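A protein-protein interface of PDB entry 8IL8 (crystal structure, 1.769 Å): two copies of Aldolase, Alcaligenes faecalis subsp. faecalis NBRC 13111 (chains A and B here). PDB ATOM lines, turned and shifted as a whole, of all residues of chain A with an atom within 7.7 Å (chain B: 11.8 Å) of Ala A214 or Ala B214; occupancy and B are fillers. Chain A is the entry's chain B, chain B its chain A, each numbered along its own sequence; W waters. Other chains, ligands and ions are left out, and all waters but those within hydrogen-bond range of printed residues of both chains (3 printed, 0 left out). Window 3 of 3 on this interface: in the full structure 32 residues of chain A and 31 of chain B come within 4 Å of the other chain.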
ATOM      1  N   TRP A 124     -14.173  -4.708 -10.779  1.00  0.00           N
ATOM      2  CA  TRP A 124     -14.778  -5.569 -11.780  1.00  0.00           C
ATOM      3  C   TRP A 124     -15.626  -4.831 -12.776  1.00  0.00           C
ATOM      4  O   TRP A 124     -15.491  -5.104 -13.969  1.00  0.00           O
ATOM      5  CB  TRP A 124     -15.526  -6.716 -11.122  1.00  0.00           C
ATOM      6  CG  TRP A 124     -14.589  -7.616 -10.363  1.00  0.00           C
ATOM      7  CD1 TRP A 124     -14.331  -7.589  -9.025  1.00  0.00           C
ATOM      8  CD2 TRP A 124     -13.746  -8.642 -10.915  1.00  0.00           C
ATOM      9  NE1 TRP A 124     -13.426  -8.578  -8.700  1.00  0.00           N
ATOM     10  CE2 TRP A 124     -13.074  -9.255  -9.837  1.00  0.00           C
ATOM     11  CE3 TRP A 124     -13.567  -9.164 -12.200  1.00  0.00           C
ATOM     12  CZ2 TRP A 124     -12.202 -10.338 -10.009  1.00  0.00           C
ATOM     13  CZ3 TRP A 124     -12.712 -10.245 -12.366  1.00  0.00           C
ATOM     14  CH2 TRP A 124     -12.011 -10.794 -11.284  1.00  0.00           C
ATOM     15  N   LEU A 208     -18.846 -11.704 -11.842  1.00  0.00           N
ATOM     16  CA  LEU A 208     -19.396 -12.984 -12.235  1.00  0.00           C
ATOM     17  C   LEU A 208     -19.227 -13.154 -13.758  1.00  0.00           C
ATOM     18  O   LEU A 208     -18.761 -14.192 -14.197  1.00  0.00           O
ATOM     19  CB  LEU A 208     -20.894 -12.989 -11.856  1.00  0.00           C
ATOM     20  CG  LEU A 208     -21.638 -14.225 -12.273  1.00  0.00           C
ATOM     21  CD1 LEU A 208     -21.088 -15.469 -11.509  1.00  0.00           C
ATOM     22  CD2 LEU A 208     -23.126 -14.050 -12.131  1.00  0.00           C
ATOM     23  N   GLN A 209     -19.587 -12.124 -14.556  1.00  0.00           N
ATOM     24  CA  GLN A 209     -19.465 -12.170 -16.009  1.00  0.00           C
ATOM     25  C   GLN A 209     -17.986 -12.288 -16.466  1.00  0.00           C
ATOM     26  O   GLN A 209     -17.700 -13.077 -17.362  1.00  0.00           O
ATOM     27  CB  GLN A 209     -20.110 -10.932 -16.621  1.00  0.00           C
ATOM     28  CG  GLN A 209     -19.860 -10.759 -18.122  1.00  0.00           C
ATOM     29  CD  GLN A 209     -20.734  -9.710 -18.767  1.00  0.00           C
ATOM     30  OE1 GLN A 209     -21.659  -9.167 -18.153  1.00  0.00           O
ATOM     31  NE2 GLN A 209     -20.466  -9.403 -20.031  1.00  0.00           N
ATOM     32  N   VAL A 210     -17.074 -11.473 -15.904  1.00  0.00           N
ATOM     33  CA  VAL A 210     -15.650 -11.542 -16.280  1.00  0.00           C
ATOM     34  C   VAL A 210     -15.081 -12.914 -15.968  1.00  0.00           C
ATOM     35  O   VAL A 210     -14.436 -13.508 -16.837  1.00  0.00           O
ATOM     36  CB  VAL A 210     -14.858 -10.393 -15.647  1.00  0.00           C
ATOM     37  CG1 VAL A 210     -13.346 -10.537 -15.882  1.00  0.00           C
ATOM     38  CG2 VAL A 210     -15.368  -9.030 -16.161  1.00  0.00           C
ATOM     39  N   ARG A 211     -15.361 -13.465 -14.761  1.00  0.00           N
ATOM     40  CA  ARG A 211     -14.846 -14.804 -14.406  1.00  0.00           C
ATOM     41  C   ARG A 211     -15.440 -15.873 -15.304  1.00  0.00           C
ATOM     42  O   ARG A 211     -14.714 -16.743 -15.752  1.00  0.00           O
ATOM     43  CB  ARG A 211     -15.143 -15.151 -12.947  1.00  0.00           C
ATOM     44  CG  ARG A 211     -14.336 -14.341 -11.963  1.00  0.00           C
ATOM     45  CD  ARG A 211     -14.896 -14.507 -10.568  1.00  0.00           C
ATOM     46  NE  ARG A 211     -13.912 -14.129  -9.556  1.00  0.00           N
ATOM     47  CZ  ARG A 211     -14.151 -14.079  -8.252  1.00  0.00           C
ATOM     48  NH1 ARG A 211     -15.331 -14.444  -7.772  1.00  0.00           N
ATOM     49  NH2 ARG A 211     -13.181 -13.752  -7.406  1.00  0.00           N
ATOM     50  N   ALA A 212     -16.757 -15.804 -15.594  1.00  0.00           N
ATOM     51  CA  ALA A 212     -17.392 -16.794 -16.465  1.00  0.00           C
ATOM     52  C   ALA A 212     -16.847 -16.732 -17.896  1.00  0.00           C
ATOM     53  O   ALA A 212     -16.544 -17.773 -18.462  1.00  0.00           O
ATOM     54  CB  ALA A 212     -18.910 -16.621 -16.471  1.00  0.00           C
ATOM     55  N   GLN A 213     -16.729 -15.524 -18.478  1.00  0.00           N
ATOM     56  CA  GLN A 213     -16.224 -15.379 -19.832  1.00  0.00           C
ATOM     57  C   GLN A 213     -14.760 -15.784 -19.981  1.00  0.00           C
ATOM     58  O   GLN A 213     -14.413 -16.370 -21.013  1.00  0.00           O
ATOM     59  CB  GLN A 213     -16.484 -13.969 -20.384  1.00  0.00           C
ATOM     60  CG  GLN A 213     -17.976 -13.717 -20.581  1.00  0.00           C
ATOM     61  CD  GLN A 213     -18.271 -12.577 -21.530  1.00  0.00           C
ATOM     62  OE1 GLN A 213     -19.023 -11.654 -21.211  1.00  0.00           O
ATOM     63  NE2 GLN A 213     -17.702 -12.625 -22.728  1.00  0.00           N
ATOM     64  N   ALA A 214     -13.900 -15.548 -18.962  1.00  0.00           N
ATOM     65  CA  ALA A 214     -12.500 -15.955 -19.052  1.00  0.00           C
ATOM     66  C   ALA A 214     -12.380 -17.476 -19.153  1.00  0.00           C
ATOM     67  O   ALA A 214     -11.546 -17.991 -19.886  1.00  0.00           O
ATOM     68  CB  ALA A 214     -11.736 -15.473 -17.832  1.00  0.00           C
ATOM     69  N   ALA A 215     -13.229 -18.203 -18.425  1.00  0.00           N
ATOM     70  CA  ALA A 215     -13.163 -19.663 -18.406  1.00  0.00           C
ATOM     71  C   ALA A 215     -13.948 -20.299 -19.529  1.00  0.00           C
ATOM     72  O   ALA A 215     -13.530 -21.331 -20.059  1.00  0.00           O
ATOM     73  CB  ALA A 215     -13.677 -20.179 -17.068  1.00  0.00           C
ATOM     74  N   PHE A 216     -15.105 -19.708 -19.886  1.00  0.00           N
ATOM     75  CA  PHE A 216     -16.025 -20.384 -20.795  1.00  0.00           C
ATOM     76  C   PHE A 216     -16.490 -19.620 -22.040  1.00  0.00           C
ATOM     77  O   PHE A 216     -17.280 -20.173 -22.807  1.00  0.00           O
ATOM     78  CB  PHE A 216     -17.263 -20.843 -19.992  1.00  0.00           C
ATOM     79  CG  PHE A 216     -16.930 -21.644 -18.742  1.00  0.00           C
ATOM     80  CD1 PHE A 216     -16.372 -22.909 -18.835  1.00  0.00           C
ATOM     81  CD2 PHE A 216     -17.166 -21.123 -17.477  1.00  0.00           C
ATOM     82  CE1 PHE A 216     -16.069 -23.642 -17.688  1.00  0.00           C
ATOM     83  CE2 PHE A 216     -16.846 -21.852 -16.338  1.00  0.00           C
ATOM     84  CZ  PHE A 216     -16.287 -23.103 -16.451  1.00  0.00           C
ATOM     85  N   GLY A 217     -16.056 -18.380 -22.225  1.00  0.00           N
ATOM     86  CA  GLY A 217     -16.496 -17.583 -23.356  1.00  0.00           C
ATOM     87  C   GLY A 217     -17.807 -16.864 -23.112  1.00  0.00           C
ATOM     88  O   GLY A 217     -18.330 -16.854 -21.992  1.00  0.00           O
ATOM     89  N   PRO A 218     -18.373 -16.283 -24.180  1.00  0.00           N
ATOM     90  CA  PRO A 218     -19.620 -15.508 -24.040  1.00  0.00           C
ATOM     91  C   PRO A 218     -20.806 -16.261 -23.423  1.00  0.00           C
ATOM     92  O   PRO A 218     -20.996 -17.450 -23.646  1.00  0.00           O
ATOM     93  CB  PRO A 218     -19.911 -15.040 -25.469  1.00  0.00           C
ATOM     94  CG  PRO A 218     -18.554 -14.985 -26.108  1.00  0.00           C
ATOM     95  CD  PRO A 218     -17.827 -16.186 -25.545  1.00  0.00           C
ATOM     96  N   TRP B 124     -18.026 -18.602  -6.844  1.00  0.00           N
ATOM     97  CA  TRP B 124     -17.472 -19.507  -7.834  1.00  0.00           C
ATOM     98  C   TRP B 124     -18.463 -20.527  -8.330  1.00  0.00           C
ATOM     99  O   TRP B 124     -18.513 -20.736  -9.542  1.00  0.00           O
ATOM    100  CB  TRP B 124     -16.196 -20.148  -7.312  1.00  0.00           C
ATOM    101  CG  TRP B 124     -15.120 -19.135  -7.088  1.00  0.00           C
ATOM    102  CD1 TRP B 124     -14.783 -18.543  -5.909  1.00  0.00           C
ATOM    103  CD2 TRP B 124     -14.270 -18.561  -8.087  1.00  0.00           C
ATOM    104  NE1 TRP B 124     -13.753 -17.663  -6.103  1.00  0.00           N
ATOM    105  CE2 TRP B 124     -13.378 -17.694  -7.424  1.00  0.00           C
ATOM    106  CE3 TRP B 124     -14.122 -18.757  -9.471  1.00  0.00           C
ATOM    107  CZ2 TRP B 124     -12.399 -16.966  -8.108  1.00  0.00           C
ATOM    108  CZ3 TRP B 124     -13.149 -18.037 -10.144  1.00  0.00           C
ATOM    109  CH2 TRP B 124     -12.316 -17.137  -9.467  1.00  0.00           C
ATOM    110  N   THR B 126     -21.550 -20.049  -8.583  1.00  0.00           N
ATOM    111  CA  THR B 126     -22.459 -19.269  -9.408  1.00  0.00           C
ATOM    112  C   THR B 126     -21.834 -18.989 -10.786  1.00  0.00           C
ATOM    113  O   THR B 126     -22.593 -18.879 -11.748  1.00  0.00           O
ATOM    114  CB  THR B 126     -22.941 -18.023  -8.639  1.00  0.00           C
ATOM    115  OG1 THR B 126     -23.642 -18.521  -7.506  1.00  0.00           O
ATOM    116  CG2 THR B 126     -23.847 -17.101  -9.454  1.00  0.00           C
ATOM    117  N   VAL B 127     -20.485 -18.974 -10.921  1.00  0.00           N
ATOM    118  CA  VAL B 127     -19.863 -18.844 -12.244  1.00  0.00           C
ATOM    119  C   VAL B 127     -20.246 -20.085 -13.095  1.00  0.00           C
ATOM    120  O   VAL B 127     -20.668 -19.936 -14.237  1.00  0.00           O
ATOM    121  CB  VAL B 127     -18.309 -18.725 -12.158  1.00  0.00           C
ATOM    122  CG1 VAL B 127     -17.687 -18.914 -13.532  1.00  0.00           C
ATOM    123  CG2 VAL B 127     -17.886 -17.387 -11.549  1.00  0.00           C
ATOM    124  N   LEU B 128     -20.114 -21.303 -12.515  1.00  0.00           N
ATOM    125  CA  LEU B 128     -20.507 -22.539 -13.184  1.00  0.00           C
ATOM    126  C   LEU B 128     -21.994 -22.490 -13.553  1.00  0.00           C
ATOM    127  O   LEU B 128     -22.367 -22.867 -14.662  1.00  0.00           O
ATOM    128  CB  LEU B 128     -20.262 -23.780 -12.282  1.00  0.00           C
ATOM    129  CG  LEU B 128     -18.808 -24.134 -11.945  1.00  0.00           C
ATOM    130  CD1 LEU B 128     -18.743 -25.516 -11.296  1.00  0.00           C
ATOM    131  CD2 LEU B 128     -17.929 -24.113 -13.173  1.00  0.00           C
ATOM    132  N   THR B 130     -23.956 -19.866 -14.022  1.00  0.00           N
ATOM    133  CA  THR B 130     -24.185 -18.808 -15.007  1.00  0.00           C
ATOM    134  C   THR B 130     -23.696 -19.205 -16.393  1.00  0.00           C
ATOM    135  O   THR B 130     -24.361 -18.925 -17.386  1.00  0.00           O
ATOM    136  CB  THR B 130     -23.534 -17.533 -14.510  1.00  0.00           C
ATOM    137  OG1 THR B 130     -24.067 -17.263 -13.211  1.00  0.00           O
ATOM    138  CG2 THR B 130     -23.752 -16.353 -15.459  1.00  0.00           C
ATOM    139  N   ALA B 131     -22.561 -19.902 -16.454  1.00  0.00           N
ATOM    140  CA  ALA B 131     -22.029 -20.388 -17.726  1.00  0.00           C
ATOM    141  C   ALA B 131     -22.668 -21.721 -18.174  1.00  0.00           C
ATOM    142  O   ALA B 131     -22.275 -22.238 -19.220  1.00  0.00           O
ATOM    143  CB  ALA B 131     -20.524 -20.548 -17.626  1.00  0.00           C
ATOM    144  N   GLN B 133     -22.334 -24.695 -16.858  1.00  0.00           N
ATOM    145  CA  GLN B 133     -21.241 -25.638 -16.867  1.00  0.00           C
ATOM    146  C   GLN B 133     -21.252 -26.548 -15.675  1.00  0.00           C
ATOM    147  O   GLN B 133     -20.961 -26.100 -14.561  1.00  0.00           O
ATOM    148  CB  GLN B 133     -19.901 -24.873 -16.885  1.00  0.00           C
ATOM    149  CG  GLN B 133     -19.666 -24.148 -18.205  1.00  0.00           C
ATOM    150  CD  GLN B 133     -19.119 -25.068 -19.283  1.00  0.00           C
ATOM    151  OE1 GLN B 133     -18.592 -26.182 -19.013  1.00  0.00           O
ATOM    152  NE2 GLN B 133     -19.214 -24.595 -20.523  1.00  0.00           N
ATOM    153  N   VAL B 136     -16.697 -30.768 -13.225  1.00  0.00           N
ATOM    154  CA  VAL B 136     -15.923 -31.855 -13.809  1.00  0.00           C
ATOM    155  C   VAL B 136     -14.958 -32.333 -12.730  1.00  0.00           C
ATOM    156  O   VAL B 136     -14.087 -31.564 -12.310  1.00  0.00           O
ATOM    157  CB  VAL B 136     -15.167 -31.390 -15.081  1.00  0.00           C
ATOM    158  CG1 VAL B 136     -14.211 -32.467 -15.586  1.00  0.00           C
ATOM    159  CG2 VAL B 136     -16.150 -30.971 -16.174  1.00  0.00           C
ATOM    160  N   ALA B 205     -14.294 -26.456  -5.347  1.00  0.00           N
ATOM    161  CA  ALA B 205     -14.155 -27.273  -6.561  1.00  0.00           C
ATOM    162  C   ALA B 205     -14.493 -26.389  -7.786  1.00  0.00           C
ATOM    163  O   ALA B 205     -13.765 -26.403  -8.780  1.00  0.00           O
ATOM    164  CB  ALA B 205     -15.080 -28.490  -6.494  1.00  0.00           C
ATOM    165  N   ALA B 206     -15.539 -25.583  -7.675  1.00  0.00           N
ATOM    166  CA  ALA B 206     -15.930 -24.676  -8.728  1.00  0.00           C
ATOM    167  C   ALA B 206     -14.824 -23.630  -8.972  1.00  0.00           C
ATOM    168  O   ALA B 206     -14.480 -23.371 -10.128  1.00  0.00           O
ATOM    169  CB  ALA B 206     -17.238 -23.986  -8.358  1.00  0.00           C
ATOM    170  N   ARG B 207     -14.233 -23.065  -7.896  1.00  0.00           N
ATOM    171  CA  ARG B 207     -13.161 -22.089  -8.055  1.00  0.00           C
ATOM    172  C   ARG B 207     -11.959 -22.711  -8.791  1.00  0.00           C
ATOM    173  O   ARG B 207     -11.356 -22.087  -9.677  1.00  0.00           O
ATOM    174  CB  ARG B 207     -12.677 -21.571  -6.685  1.00  0.00           C
ATOM    175  CG  ARG B 207     -11.498 -20.615  -6.809  1.00  0.00           C
ATOM    176  CD  ARG B 207     -11.217 -19.973  -5.506  1.00  0.00           C
ATOM    177  NE  ARG B 207     -10.647 -20.929  -4.559  1.00  0.00           N
ATOM    178  CZ  ARG B 207     -10.336 -20.620  -3.306  1.00  0.00           C
ATOM    179  NH1 ARG B 207     -10.539 -19.383  -2.845  1.00  0.00           N
ATOM    180  NH2 ARG B 207      -9.808 -21.528  -2.509  1.00  0.00           N
ATOM    181  N   LEU B 208     -11.621 -23.941  -8.395  1.00  0.00           N
ATOM    182  CA  LEU B 208     -10.509 -24.668  -8.964  1.00  0.00           C
ATOM    183  C   LEU B 208     -10.745 -24.919 -10.460  1.00  0.00           C
ATOM    184  O   LEU B 208      -9.870 -24.664 -11.264  1.00  0.00           O
ATOM    185  CB  LEU B 208     -10.373 -25.998  -8.194  1.00  0.00           C
ATOM    186  CG  LEU B 208      -9.278 -26.894  -8.675  1.00  0.00           C
ATOM    187  CD1 LEU B 208      -7.937 -26.246  -8.471  1.00  0.00           C
ATOM    188  CD2 LEU B 208      -9.394 -28.283  -8.030  1.00  0.00           C
ATOM    189  N   GLN B 209     -11.946 -25.361 -10.829  1.00  0.00           N
ATOM    190  CA  GLN B 209     -12.299 -25.621 -12.219  1.00  0.00           C
ATOM    191  C   GLN B 209     -12.329 -24.334 -13.075  1.00  0.00           C
ATOM    192  O   GLN B 209     -11.854 -24.347 -14.204  1.00  0.00           O
ATOM    193  CB  GLN B 209     -13.672 -26.319 -12.274  1.00  0.00           C
ATOM    194  CG  GLN B 209     -14.224 -26.479 -13.673  1.00  0.00           C
ATOM    195  CD  GLN B 209     -15.420 -27.394 -13.760  1.00  0.00           C
ATOM    196  OE1 GLN B 209     -15.767 -28.101 -12.801  1.00  0.00           O
ATOM    197  NE2 GLN B 209     -16.058 -27.427 -14.929  1.00  0.00           N
ATOM    198  N   VAL B 210     -12.921 -23.253 -12.569  1.00  0.00           N
ATOM    199  CA  VAL B 210     -12.978 -21.993 -13.330  1.00  0.00           C
ATOM    200  C   VAL B 210     -11.562 -21.454 -13.559  1.00  0.00           C
ATOM    201  O   VAL B 210     -11.224 -21.096 -14.696  1.00  0.00           O
ATOM    202  CB  VAL B 210     -13.903 -20.972 -12.659  1.00  0.00           C
ATOM    203  CG1 VAL B 210     -13.811 -19.583 -13.336  1.00  0.00           C
ATOM    204  CG2 VAL B 210     -15.351 -21.491 -12.636  1.00  0.00           C
ATOM    205  N   ARG B 211     -10.706 -21.464 -12.518  1.00  0.00           N
ATOM    206  CA  ARG B 211      -9.330 -20.977 -12.685  1.00  0.00           C
ATOM    207  C   ARG B 211      -8.550 -21.862 -13.659  1.00  0.00           C
ATOM    208  O   ARG B 211      -7.833 -21.350 -14.501  1.00  0.00           O
ATOM    209  CB  ARG B 211      -8.593 -20.909 -11.338  1.00  0.00           C
ATOM    210  CG  ARG B 211      -9.103 -19.822 -10.425  1.00  0.00           C
ATOM    211  CD  ARG B 211      -8.574 -20.026  -9.029  1.00  0.00           C
ATOM    212  NE  ARG B 211      -8.651 -18.793  -8.256  1.00  0.00           N
ATOM    213  CZ  ARG B 211      -8.288 -18.675  -6.982  1.00  0.00           C
ATOM    214  NH1 ARG B 211      -7.818 -19.733  -6.313  1.00  0.00           N
ATOM    215  NH2 ARG B 211      -8.331 -17.490  -6.379  1.00  0.00           N
ATOM    216  N   ALA B 212      -8.678 -23.187 -13.540  1.00  0.00           N
ATOM    217  CA  ALA B 212      -7.979 -24.102 -14.438  1.00  0.00           C
ATOM    218  C   ALA B 212      -8.448 -23.947 -15.895  1.00  0.00           C
ATOM    219  O   ALA B 212      -7.614 -23.888 -16.787  1.00  0.00           O
ATOM    220  CB  ALA B 212      -8.152 -25.551 -13.970  1.00  0.00           C
ATOM    221  N   GLN B 213      -9.775 -23.908 -16.136  1.00  0.00           N
ATOM    222  CA  GLN B 213     -10.293 -23.778 -17.485  1.00  0.00           C
ATOM    223  C   GLN B 213      -9.954 -22.425 -18.137  1.00  0.00           C
ATOM    224  O   GLN B 213      -9.677 -22.409 -19.336  1.00  0.00           O
ATOM    225  CB  GLN B 213     -11.798 -24.073 -17.535  1.00  0.00           C
ATOM    226  CG  GLN B 213     -12.089 -25.540 -17.252  1.00  0.00           C
ATOM    227  CD  GLN B 213     -13.450 -25.966 -17.747  1.00  0.00           C
ATOM    228  OE1 GLN B 213     -14.234 -26.533 -17.005  1.00  0.00           O
ATOM    229  NE2 GLN B 213     -13.758 -25.722 -19.013  1.00  0.00           N
ATOM    230  N   ALA B 214      -9.884 -21.321 -17.361  1.00  0.00           N
ATOM    231  CA  ALA B 214      -9.527 -20.020 -17.933  1.00  0.00           C
ATOM    232  C   ALA B 214      -8.106 -20.032 -18.476  1.00  0.00           C
ATOM    233  O   ALA B 214      -7.842 -19.449 -19.523  1.00  0.00           O
ATOM    234  CB  ALA B 214      -9.671 -18.926 -16.900  1.00  0.00           C
ATOM    235  N   ALA B 215      -7.190 -20.715 -17.782  1.00  0.00           N
ATOM    236  CA  ALA B 215      -5.803 -20.768 -18.209  1.00  0.00           C
ATOM    237  C   ALA B 215      -5.521 -21.875 -19.198  1.00  0.00           C
ATOM    238  O   ALA B 215      -4.655 -21.713 -20.057  1.00  0.00           O
ATOM    239  CB  ALA B 215      -4.891 -20.927 -16.989  1.00  0.00           C
ATOM    240  N   PHE B 216      -6.186 -23.030 -19.045  1.00  0.00           N
ATOM    241  CA  PHE B 216      -5.795 -24.225 -19.800  1.00  0.00           C
ATOM    242  C   PHE B 216      -6.877 -24.958 -20.591  1.00  0.00           C
ATOM    243  O   PHE B 216      -6.563 -25.960 -21.232  1.00  0.00           O
ATOM    244  CB  PHE B 216      -5.124 -25.232 -18.837  1.00  0.00           C
ATOM    245  CG  PHE B 216      -3.997 -24.652 -18.003  1.00  0.00           C
ATOM    246  CD1 PHE B 216      -2.816 -24.242 -18.593  1.00  0.00           C
ATOM    247  CD2 PHE B 216      -4.137 -24.490 -16.630  1.00  0.00           C
ATOM    248  CE1 PHE B 216      -1.771 -23.728 -17.819  1.00  0.00           C
ATOM    249  CE2 PHE B 216      -3.111 -23.945 -15.862  1.00  0.00           C
ATOM    250  CZ  PHE B 216      -1.940 -23.545 -16.462  1.00  0.00           C
ATOM    251  N   GLY B 217      -8.111 -24.487 -20.554  1.00  0.00           N
ATOM    252  CA  GLY B 217      -9.204 -25.127 -21.269  1.00  0.00           C
ATOM    253  C   GLY B 217      -9.826 -26.275 -20.501  1.00  0.00           C
ATOM    254  O   GLY B 217      -9.534 -26.481 -19.318  1.00  0.00           O
ATOM    255  N   PRO B 218     -10.683 -27.060 -21.183  1.00  0.00           N
ATOM    256  CA  PRO B 218     -11.386 -28.164 -20.506  1.00  0.00           C
ATOM    257  C   PRO B 218     -10.498 -29.194 -19.820  1.00  0.00           C
ATOM    258  O   PRO B 218      -9.426 -29.539 -20.308  1.00  0.00           O
ATOM    259  CB  PRO B 218     -12.237 -28.772 -21.616  1.00  0.00           C
ATOM    260  CG  PRO B 218     -12.495 -27.615 -22.545  1.00  0.00           C
ATOM    261  CD  PRO B 218     -11.167 -26.889 -22.565  1.00  0.00           C
ATOM    262  N   LEU B 219     -10.947 -29.634 -18.639  1.00  0.00           N
ATOM    263  CA  LEU B 219     -10.247 -30.575 -17.776  1.00  0.00           C
ATOM    264  C   LEU B 219     -10.455 -32.013 -18.173  1.00  0.00           C
ATOM    265  O   LEU B 219     -11.475 -32.359 -18.747  1.00  0.00           O
ATOM    266  CB  LEU B 219     -10.742 -30.415 -16.328  1.00  0.00           C
ATOM    267  CG  LEU B 219     -10.641 -29.036 -15.691  1.00  0.00           C
ATOM    268  CD1 LEU B 219     -11.300 -29.044 -14.326  1.00  0.00           C
ATOM    269  CD2 LEU B 219      -9.204 -28.612 -15.555  1.00  0.00           C
ATOM    270  N   THR B 220      -9.500 -32.862 -17.819  1.00  0.00           N
ATOM    271  CA  THR B 220      -9.550 -34.305 -18.002  1.00  0.00           C
ATOM    272  C   THR B 220     -10.074 -34.810 -16.664  1.00  0.00           C
ATOM    273  O   THR B 220      -9.479 -34.524 -15.615  1.00  0.00           O
ATOM    274  CB  THR B 220      -8.118 -34.868 -18.212  1.00  0.00           C
ATOM    275  OG1 THR B 220      -7.635 -34.499 -19.507  1.00  0.00           O
ATOM    276  CG2 THR B 220      -8.047 -36.395 -18.034  1.00  0.00           C
HETATM  277  O   HOH W   1     -12.872 -23.530 -21.104  1.00  0.00           O
HETATM  278  O   HOH W   2     -10.495 -20.821 -21.699  1.00  0.00           O
HETATM  279  O   HOH W   3      -9.003 -16.921 -20.300  1.00  0.00           O
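The side-chain hydroxyl (OG1) of Thr B130 lies within hydrogen-bond range of the backbone carbonyl oxygen (O) of Thr B126 (2.6 Å). The backbone carbonyl oxygen of Leu B128 sits at hydrogen-bond distance from the backbone NH of Gln B133, 2.9 Å away. NE2 of Gln B209 sits at hydrogen-bond distance from OE1 of Gln B213, at 2.9 Å.
Leu A208 touches Val B127. CD2 of Leu A208 touches OG1 of Thr B130, 3.5 Å away. CZ of Arg A211 touches CZ2 of Trp B124 (3.4 Å). Val B127 touches Arg A211. Val B210 touches Arg A211 (CG1 to O, 3.8 Å). CA of Ala A212 touches CG1 of Val B127, at 3.6 Å. Ala A215 touches Ala B214 (CA to CA, 3.7 Å). Phe A216 touches Leu B128. Ala B131 touches Phe A216 (CB to CD2, 3.4 Å). NE2 of Gln B213 touches CE1 of Phe A216, 3.4 Å away.
No residue of chain B comes within 4 Å of Val A210. Of the printed residues of chain B, Arg A211 touches Trp B124 (3.4 Å), Val B127 (3.8 Å) and Val B210 (3.8 Å). Of chain B, only Val B127 (3.6 Å) comes within 4 Å of Ala A212. Of chain B, only Val B210 (3.5 Å) and Ala B214 (3.7 Å) come within 4 Å of Ala A215. Of the printed residues of chain B, Phe A216 touches Leu B128, Ala B131, Gln B133 and Gln B213. Printed residues of chain A within 4 Å of Trp B124: Arg A211 (3.4 Å). Printed residues of chain A within 4 Å of Gln B133: Phe A216 (3.5 Å). Ala B214 touches two residues of chain A. The nearest residue of chain A that does not touch Ala B214 is Arg A211 (5.6 Å). The nearest printed residue of chain B that does not touch Arg A211 is Ala B214 (5.6 Å).
Of the 12 printed residues of chain A, 6 touch a printed residue of chain B. Along chain A the printed residues that touch a printed residue of chain B span positions 208 to 216. Along chain B the printed residues that touch a printed residue of chain A span positions 124 to 214. Among the printed residues, 14 pairs touch across the chains. Among the printed residues, no Asp or Glu carboxylate lies within 4 Å of a Lys or Arg side-chain nitrogen of the other chain.
Arg A211 touches Val B210, but with the chains exchanged Val A210 does not touch Arg B211 (9.8 Å). Ala A214 touches its own counterpart, Ala B214. Ala A215 touches Val B210, but with the chains exchanged Val A210 does not touch Ala B215 (10.3 Å). Ala A215 touches Ala B214, but with the chains exchanged Ala A214 does not touch Ala B215 (5.6 Å). Positions printed for both chains: 124, 208, 209, 210, 211, 212, 213, 214, 215, 216, 217 and 218. Of the 14 pairs that touch across the chains among the printed residues, 1 has its exchanged pair printed and touching as well.
Water W1 lies within hydrogen-bond range of O of Ala A215 (2.5 Å) and NE2 of Gln B213 (3.2 Å). Water W3 lies within hydrogen-bond range of O of Ala A214 (2.8 Å) and O of Ala B214 (2.9 Å). Water W2 lies within hydrogen-bond range of O of Gln B213 (3.0 Å) and O of Ala A215 (3.5 Å).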
